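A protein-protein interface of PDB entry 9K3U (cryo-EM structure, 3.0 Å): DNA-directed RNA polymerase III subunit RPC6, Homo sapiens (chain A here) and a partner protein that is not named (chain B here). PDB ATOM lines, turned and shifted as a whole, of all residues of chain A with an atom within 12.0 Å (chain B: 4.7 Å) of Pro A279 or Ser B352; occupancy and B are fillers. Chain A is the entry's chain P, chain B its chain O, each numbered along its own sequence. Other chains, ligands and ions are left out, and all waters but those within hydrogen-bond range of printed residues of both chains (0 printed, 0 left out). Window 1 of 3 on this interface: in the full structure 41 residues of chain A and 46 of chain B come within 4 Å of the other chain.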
ATOM      1  N   ILE A 243      19.228 -24.363 -14.352  1.00  0.00           N
ATOM      2  CA  ILE A 243      17.902 -24.489 -13.749  1.00  0.00           C
ATOM      3  C   ILE A 243      17.791 -25.804 -12.990  1.00  0.00           C
ATOM      4  O   ILE A 243      17.391 -25.834 -11.820  1.00  0.00           O
ATOM      5  CB  ILE A 243      16.808 -24.371 -14.828  1.00  0.00           C
ATOM      6  CG1 ILE A 243      16.800 -22.963 -15.427  1.00  0.00           C
ATOM      7  CG2 ILE A 243      15.443 -24.713 -14.240  1.00  0.00           C
ATOM      8  CD1 ILE A 243      15.934 -22.827 -16.657  1.00  0.00           C
ATOM      9  N   TYR A 244      18.141 -26.911 -13.648  1.00  0.00           N
ATOM     10  CA  TYR A 244      18.127 -28.208 -12.981  1.00  0.00           C
ATOM     11  C   TYR A 244      18.995 -28.209 -11.730  1.00  0.00           C
ATOM     12  O   TYR A 244      18.700 -28.946 -10.784  1.00  0.00           O
ATOM     13  CB  TYR A 244      18.603 -29.298 -13.945  1.00  0.00           C
ATOM     14  CG  TYR A 244      17.814 -29.368 -15.235  1.00  0.00           C
ATOM     15  CD1 TYR A 244      16.461 -29.052 -15.263  1.00  0.00           C
ATOM     16  CD2 TYR A 244      18.424 -29.744 -16.424  1.00  0.00           C
ATOM     17  CE1 TYR A 244      15.741 -29.114 -16.440  1.00  0.00           C
ATOM     18  CE2 TYR A 244      17.710 -29.809 -17.604  1.00  0.00           C
ATOM     19  CZ  TYR A 244      16.367 -29.492 -17.607  1.00  0.00           C
ATOM     20  OH  TYR A 244      15.652 -29.555 -18.781  1.00  0.00           O
ATOM     21  N   ASP A 245      20.054 -27.406 -11.705  1.00  0.00           N
ATOM     22  CA  ASP A 245      20.883 -27.262 -10.516  1.00  0.00           C
ATOM     23  C   ASP A 245      20.167 -26.530  -9.387  1.00  0.00           C
ATOM     24  O   ASP A 245      20.640 -26.572  -8.245  1.00  0.00           O
ATOM     25  CB  ASP A 245      22.179 -26.525 -10.868  1.00  0.00           C
ATOM     26  CG  ASP A 245      23.214 -26.600  -9.761  1.00  0.00           C
ATOM     27  OD1 ASP A 245      23.008 -27.369  -8.798  1.00  0.00           O
ATOM     28  OD2 ASP A 245      24.235 -25.885  -9.854  1.00  0.00           O
ATOM     29  N   GLY A 246      19.047 -25.871  -9.671  1.00  0.00           N
ATOM     30  CA  GLY A 246      18.300 -25.180  -8.636  1.00  0.00           C
ATOM     31  C   GLY A 246      18.853 -23.821  -8.269  1.00  0.00           C
ATOM     32  O   GLY A 246      18.951 -23.502  -7.080  1.00  0.00           O
ATOM     33  N   LYS A 247      19.219 -23.007  -9.263  1.00  0.00           N
ATOM     34  CA  LYS A 247      19.796 -21.692  -9.017  1.00  0.00           C
ATOM     35  C   LYS A 247      19.185 -20.584  -9.864  1.00  0.00           C
ATOM     36  O   LYS A 247      19.250 -19.418  -9.459  1.00  0.00           O
ATOM     37  CB  LYS A 247      21.312 -21.726  -9.265  1.00  0.00           C
ATOM     38  CG  LYS A 247      22.038 -22.801  -8.460  1.00  0.00           C
ATOM     39  CD  LYS A 247      23.474 -22.995  -8.918  1.00  0.00           C
ATOM     40  CE  LYS A 247      24.338 -21.790  -8.589  1.00  0.00           C
ATOM     41  NZ  LYS A 247      25.751 -21.991  -9.008  1.00  0.00           N
ATOM     42  N   ASN A 274      17.207 -17.112  -5.512  1.00  0.00           N
ATOM     43  CA  ASN A 274      17.724 -17.735  -4.305  1.00  0.00           C
ATOM     44  C   ASN A 274      16.962 -19.025  -4.009  1.00  0.00           C
ATOM     45  O   ASN A 274      15.826 -19.203  -4.457  1.00  0.00           O
ATOM     46  CB  ASN A 274      17.608 -16.771  -3.129  1.00  0.00           C
ATOM     47  CG  ASN A 274      18.406 -15.498  -3.337  1.00  0.00           C
ATOM     48  OD1 ASN A 274      19.439 -15.500  -4.004  1.00  0.00           O
ATOM     49  ND2 ASN A 274      17.926 -14.399  -2.763  1.00  0.00           N
ATOM     50  N   PRO A 275      17.567 -19.942  -3.253  1.00  0.00           N
ATOM     51  CA  PRO A 275      16.878 -21.197  -2.939  1.00  0.00           C
ATOM     52  C   PRO A 275      15.613 -20.959  -2.130  1.00  0.00           C
ATOM     53  O   PRO A 275      15.400 -19.894  -1.547  1.00  0.00           O
ATOM     54  CB  PRO A 275      17.918 -21.987  -2.136  1.00  0.00           C
ATOM     55  CG  PRO A 275      18.867 -20.960  -1.618  1.00  0.00           C
ATOM     56  CD  PRO A 275      18.915 -19.892  -2.664  1.00  0.00           C
ATOM     57  N   ILE A 276      14.758 -21.984  -2.103  1.00  0.00           N
ATOM     58  CA  ILE A 276      13.480 -21.874  -1.405  1.00  0.00           C
ATOM     59  C   ILE A 276      13.708 -21.760   0.099  1.00  0.00           C
ATOM     60  O   ILE A 276      13.231 -20.820   0.748  1.00  0.00           O
ATOM     61  CB  ILE A 276      12.575 -23.071  -1.747  1.00  0.00           C
ATOM     62  CG1 ILE A 276      12.273 -23.097  -3.249  1.00  0.00           C
ATOM     63  CG2 ILE A 276      11.283 -22.999  -0.943  1.00  0.00           C
ATOM     64  CD1 ILE A 276      11.667 -24.396  -3.738  1.00  0.00           C
ATOM     65  N   ILE A 277      14.437 -22.712   0.673  1.00  0.00           N
ATOM     66  CA  ILE A 277      14.741 -22.704   2.101  1.00  0.00           C
ATOM     67  C   ILE A 277      16.214 -23.041   2.299  1.00  0.00           C
ATOM     68  O   ILE A 277      16.808 -23.722   1.451  1.00  0.00           O
ATOM     69  CB  ILE A 277      13.843 -23.687   2.870  1.00  0.00           C
ATOM     70  CG1 ILE A 277      13.904 -25.078   2.230  1.00  0.00           C
ATOM     71  CG2 ILE A 277      12.412 -23.173   2.920  1.00  0.00           C
ATOM     72  CD1 ILE A 277      13.119 -26.135   2.980  1.00  0.00           C
ATOM     73  N   PRO A 278      16.841 -22.597   3.384  1.00  0.00           N
ATOM     74  CA  PRO A 278      18.242 -22.961   3.633  1.00  0.00           C
ATOM     75  C   PRO A 278      18.379 -24.452   3.885  1.00  0.00           C
ATOM     76  O   PRO A 278      17.379 -25.184   3.889  1.00  0.00           O
ATOM     77  CB  PRO A 278      18.609 -22.147   4.885  1.00  0.00           C
ATOM     78  CG  PRO A 278      17.577 -21.075   4.977  1.00  0.00           C
ATOM     79  CD  PRO A 278      16.331 -21.662   4.403  1.00  0.00           C
ATOM     80  N   PRO A 279      19.602 -24.941   4.093  1.00  0.00           N
ATOM     81  CA  PRO A 279      19.778 -26.365   4.399  1.00  0.00           C
ATOM     82  C   PRO A 279      18.948 -26.783   5.602  1.00  0.00           C
ATOM     83  O   PRO A 279      18.887 -26.080   6.615  1.00  0.00           O
ATOM     84  CB  PRO A 279      21.279 -26.484   4.678  1.00  0.00           C
ATOM     85  CG  PRO A 279      21.894 -25.341   3.941  1.00  0.00           C
ATOM     86  CD  PRO A 279      20.889 -24.229   4.000  1.00  0.00           C
ATOM     87  N   THR A 280      18.304 -27.941   5.483  1.00  0.00           N
ATOM     88  CA  THR A 280      17.433 -28.432   6.540  1.00  0.00           C
ATOM     89  C   THR A 280      18.258 -28.922   7.731  1.00  0.00           C
ATOM     90  O   THR A 280      19.491 -28.880   7.734  1.00  0.00           O
ATOM     91  CB  THR A 280      16.538 -29.554   6.015  1.00  0.00           C
ATOM     92  OG1 THR A 280      17.349 -30.623   5.513  1.00  0.00           O
ATOM     93  CG2 THR A 280      15.635 -29.036   4.904  1.00  0.00           C
ATOM     94  N   GLY A 281      17.547 -29.390   8.760  1.00  0.00           N
ATOM     95  CA  GLY A 281      18.207 -29.859   9.968  1.00  0.00           C
ATOM     96  C   GLY A 281      18.746 -31.268   9.887  1.00  0.00           C
ATOM     97  O   GLY A 281      19.713 -31.589  10.588  1.00  0.00           O
ATOM     98  N   LEU A 282      18.146 -32.121   9.053  1.00  0.00           N
ATOM     99  CA  LEU A 282      18.628 -33.491   8.930  1.00  0.00           C
ATOM    100  C   LEU A 282      20.071 -33.528   8.448  1.00  0.00           C
ATOM    101  O   LEU A 282      20.886 -34.308   8.956  1.00  0.00           O
ATOM    102  CB  LEU A 282      17.727 -34.280   7.979  1.00  0.00           C
ATOM    103  CG  LEU A 282      18.139 -35.731   7.713  1.00  0.00           C
ATOM    104  CD1 LEU A 282      18.096 -36.553   8.992  1.00  0.00           C
ATOM    105  CD2 LEU A 282      17.256 -36.347   6.642  1.00  0.00           C
ATOM    106  N   VAL A 283      20.409 -32.687   7.466  1.00  0.00           N
ATOM    107  CA  VAL A 283      21.760 -32.671   6.918  1.00  0.00           C
ATOM    108  C   VAL A 283      22.791 -32.180   7.921  1.00  0.00           C
ATOM    109  O   VAL A 283      23.987 -32.436   7.740  1.00  0.00           O
ATOM    110  CB  VAL A 283      21.816 -31.791   5.652  1.00  0.00           C
ATOM    111  CG1 VAL A 283      20.781 -32.252   4.637  1.00  0.00           C
ATOM    112  CG2 VAL A 283      21.611 -30.324   6.006  1.00  0.00           C
ATOM    113  N   ARG A 284      22.362 -31.482   8.971  1.00  0.00           N
ATOM    114  CA  ARG A 284      23.275 -30.973   9.984  1.00  0.00           C
ATOM    115  C   ARG A 284      23.688 -32.030  10.998  1.00  0.00           C
ATOM    116  O   ARG A 284      24.515 -31.736  11.869  1.00  0.00           O
ATOM    117  CB  ARG A 284      22.636 -29.786  10.710  1.00  0.00           C
ATOM    118  CG  ARG A 284      22.337 -28.598   9.808  1.00  0.00           C
ATOM    119  CD  ARG A 284      21.798 -27.420  10.599  1.00  0.00           C
ATOM    120  NE  ARG A 284      21.715 -26.203   9.792  1.00  0.00           N
ATOM    121  CZ  ARG A 284      20.646 -25.821   9.100  1.00  0.00           C
ATOM    122  NH1 ARG A 284      19.540 -26.554   9.105  1.00  0.00           N
ATOM    123  NH2 ARG A 284      20.681 -24.695   8.401  1.00  0.00           N
ATOM    124  N   ALA A 285      23.135 -33.246  10.913  1.00  0.00           N
ATOM    125  CA  ALA A 285      23.488 -34.328  11.817  1.00  0.00           C
ATOM    126  C   ALA A 285      24.200 -35.445  11.062  1.00  0.00           C
ATOM    127  O   ALA A 285      23.818 -35.759   9.929  1.00  0.00           O
ATOM    128  CB  ALA A 285      22.242 -34.897  12.505  1.00  0.00           C
ATOM    129  N   GLY A 288      21.967 -38.263   9.290  1.00  0.00           N
ATOM    130  CA  GLY A 288      21.286 -38.069   8.022  1.00  0.00           C
ATOM    131  C   GLY A 288      22.167 -38.237   6.804  1.00  0.00           C
ATOM    132  O   GLY A 288      21.652 -38.521   5.718  1.00  0.00           O
ATOM    133  N   LEU A 289      23.479 -38.068   6.960  1.00  0.00           N
ATOM    134  CA  LEU A 289      24.426 -38.198   5.859  1.00  0.00           C
ATOM    135  C   LEU A 289      25.279 -39.456   5.974  1.00  0.00           C
ATOM    136  O   LEU A 289      26.343 -39.530   5.352  1.00  0.00           O
ATOM    137  CB  LEU A 289      25.326 -36.964   5.791  1.00  0.00           C
ATOM    138  CG  LEU A 289      24.608 -35.611   5.813  1.00  0.00           C
ATOM    139  CD1 LEU A 289      25.610 -34.474   5.702  1.00  0.00           C
ATOM    140  CD2 LEU A 289      23.570 -35.525   4.703  1.00  0.00           C
ATOM    141  N   ALA B 348      11.693 -28.802  -1.721  1.00  0.00           N
ATOM    142  CA  ALA B 348      12.910 -28.076  -1.379  1.00  0.00           C
ATOM    143  C   ALA B 348      13.741 -28.847  -0.362  1.00  0.00           C
ATOM    144  O   ALA B 348      14.958 -28.986  -0.519  1.00  0.00           O
ATOM    145  CB  ALA B 348      12.562 -26.688  -0.843  1.00  0.00           C
ATOM    146  N   THR B 349      13.096 -29.352   0.693  1.00  0.00           N
ATOM    147  CA  THR B 349      13.810 -30.151   1.685  1.00  0.00           C
ATOM    148  C   THR B 349      14.452 -31.377   1.044  1.00  0.00           C
ATOM    149  O   THR B 349      15.610 -31.705   1.334  1.00  0.00           O
ATOM    150  CB  THR B 349      12.853 -30.571   2.803  1.00  0.00           C
ATOM    151  OG1 THR B 349      12.588 -29.452   3.655  1.00  0.00           O
ATOM    152  CG2 THR B 349      13.442 -31.715   3.621  1.00  0.00           C
ATOM    153  N   LEU B 350      13.712 -32.069   0.176  1.00  0.00           N
ATOM    154  CA  LEU B 350      14.236 -33.285  -0.433  1.00  0.00           C
ATOM    155  C   LEU B 350      15.438 -32.984  -1.321  1.00  0.00           C
ATOM    156  O   LEU B 350      16.468 -33.665  -1.233  1.00  0.00           O
ATOM    157  CB  LEU B 350      13.134 -33.983  -1.232  1.00  0.00           C
ATOM    158  CG  LEU B 350      13.459 -35.368  -1.791  1.00  0.00           C
ATOM    159  CD1 LEU B 350      13.932 -36.311  -0.693  1.00  0.00           C
ATOM    160  CD2 LEU B 350      12.242 -35.947  -2.498  1.00  0.00           C
ATOM    161  N   GLU B 351      15.332 -31.963  -2.176  1.00  0.00           N
ATOM    162  CA  GLU B 351      16.461 -31.616  -3.034  1.00  0.00           C
ATOM    163  C   GLU B 351      17.651 -31.128  -2.220  1.00  0.00           C
ATOM    164  O   GLU B 351      18.800 -31.420  -2.572  1.00  0.00           O
ATOM    165  CB  GLU B 351      16.043 -30.559  -4.057  1.00  0.00           C
ATOM    166  CG  GLU B 351      15.641 -29.228  -3.450  1.00  0.00           C
ATOM    167  CD  GLU B 351      15.132 -28.243  -4.485  1.00  0.00           C
ATOM    168  OE1 GLU B 351      15.067 -28.612  -5.675  1.00  0.00           O
ATOM    169  OE2 GLU B 351      14.796 -27.103  -4.104  1.00  0.00           O
ATOM    170  N   SER B 352      17.405 -30.408  -1.120  1.00  0.00           N
ATOM    171  CA  SER B 352      18.510 -29.937  -0.292  1.00  0.00           C
ATOM    172  C   SER B 352      19.235 -31.100   0.375  1.00  0.00           C
ATOM    173  O   SER B 352      20.471 -31.131   0.411  1.00  0.00           O
ATOM    174  CB  SER B 352      17.994 -28.955   0.758  1.00  0.00           C
ATOM    175  OG  SER B 352      19.050 -28.490   1.583  1.00  0.00           O
ATOM    176  N   VAL B 353      18.485 -32.067   0.911  1.00  0.00           N
ATOM    177  CA  VAL B 353      19.137 -33.213   1.537  1.00  0.00           C
ATOM    178  C   VAL B 353      19.870 -34.043   0.490  1.00  0.00           C
ATOM    179  O   VAL B 353      20.961 -34.562   0.755  1.00  0.00           O
ATOM    180  CB  VAL B 353      18.117 -34.050   2.336  1.00  0.00           C
ATOM    181  CG1 VAL B 353      17.063 -34.659   1.427  1.00  0.00           C
ATOM    182  CG2 VAL B 353      18.827 -35.131   3.155  1.00  0.00           C
ATOM    183  N   VAL B 354      19.310 -34.167  -0.715  1.00  0.00           N
ATOM    184  CA  VAL B 354      20.011 -34.884  -1.778  1.00  0.00           C
ATOM    185  C   VAL B 354      21.319 -34.179  -2.117  1.00  0.00           C
ATOM    186  O   VAL B 354      22.362 -34.821  -2.288  1.00  0.00           O
ATOM    187  CB  VAL B 354      19.104 -35.025  -3.015  1.00  0.00           C
ATOM    188  CG1 VAL B 354      19.913 -35.481  -4.227  1.00  0.00           C
ATOM    189  CG2 VAL B 354      17.966 -35.999  -2.731  1.00  0.00           C
ATOM    190  N   GLN B 355      21.284 -32.849  -2.220  1.00  0.00           N
ATOM    191  CA  GLN B 355      22.495 -32.097  -2.531  1.00  0.00           C
ATOM    192  C   GLN B 355      23.544 -32.268  -1.440  1.00  0.00           C
ATOM    193  O   GLN B 355      24.730 -32.460  -1.731  1.00  0.00           O
ATOM    194  CB  GLN B 355      22.158 -30.618  -2.718  1.00  0.00           C
ATOM    195  CG  GLN B 355      23.336 -29.756  -3.146  1.00  0.00           C
ATOM    196  CD  GLN B 355      22.953 -28.301  -3.340  1.00  0.00           C
ATOM    197  OE1 GLN B 355      21.786 -27.935  -3.222  1.00  0.00           O
ATOM    198  NE2 GLN B 355      23.943 -27.466  -3.640  1.00  0.00           N
ATOM    199  N   GLU B 356      23.126 -32.199  -0.175  1.00  0.00           N
ATOM    200  CA  GLU B 356      24.066 -32.313   0.930  1.00  0.00           C
ATOM    201  C   GLU B 356      24.592 -33.730   1.114  1.00  0.00           C
ATOM    202  O   GLU B 356      25.678 -33.904   1.677  1.00  0.00           O
ATOM    203  CB  GLU B 356      23.411 -31.844   2.229  1.00  0.00           C
ATOM    204  CG  GLU B 356      23.023 -30.372   2.234  1.00  0.00           C
ATOM    205  CD  GLU B 356      24.224 -29.450   2.184  1.00  0.00           C
ATOM    206  OE1 GLU B 356      25.363 -29.942   2.330  1.00  0.00           O
ATOM    207  OE2 GLU B 356      24.030 -28.229   1.993  1.00  0.00           O
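O of Pro A279 sits at hydrogen-bond distance from NH1 of Arg A284 (2.6 Å). O of Thr A280 sits at hydrogen-bond distance from NH1 of Arg A284, 2.7 Å away.
Among the printed residues, pairs that only touch across the chains: Ile A276 with Ala B348 (3.7 Å), Ile A277 with Ala B348 (3.7 Å), Ile A277 with Thr B349 (3.4 Å), Pro A279 with Ser B352 (3.6 Å), Thr A280 with Thr B349 (3.3 Å), Val A283 with Val B353 (3.6 Å) and Val A283 with Glu B356 (3.6 Å).
Lys A247 touches none of the printed residues of chain B. Printed residues of chain B within 4 Å of Ile A276: Ala B348. Of the printed residues of chain B, Ile A277 touches Ala B348 (3.7 Å) and Thr B349 (3.4 Å). Of chain B, only Ser B352 (3.6 Å) comes within 4 Å of Pro A279. Of the printed residues of chain B, Thr A280 touches Thr B349. Of the printed residues of chain B, Val A283 touches Val B353 and Glu B356. Of chain A, only Ile A276 (3.7 Å) and Ile A277 (3.7 Å) come within 4 Å of Ala B348. Of chain A, only Ile A277 and Thr A280 come within 4 Å of Thr B349. Leu B350 touches none of the printed residues of chain A. No residue of chain A comes within 4 Å of Glu B351. Printed residues of chain A within 4 Å of Ser B352: Pro A279 (3.6 Å). Of the printed residues of chain A, Val B353 touches Val A283. No residue of chain A comes within 4 Å of Gln B355. Glu B356 touches just one residue of chain A: Val A283. The nearest printed residue of chain A that does not touch Ser B352 is Thr A280 (4.01 Å).
Hydrophobic or aromatic side chains of chain B within 4 Å of the printed part of chain A: Ala B348 and Val B353. Printed residues of chain A that touch a printed residue of chain B: Ile A276, Ile A277, Pro A279, Thr A280 and Val A283. Hydrophobic or aromatic side chains of chain A that line the printed part of chain B: Ile A276, Ile A277 and Val A283. Among the printed residues, no Asp or Glu carboxylate lies within 4 Å of a Lys or Arg side-chain nitrogen of the other chain.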
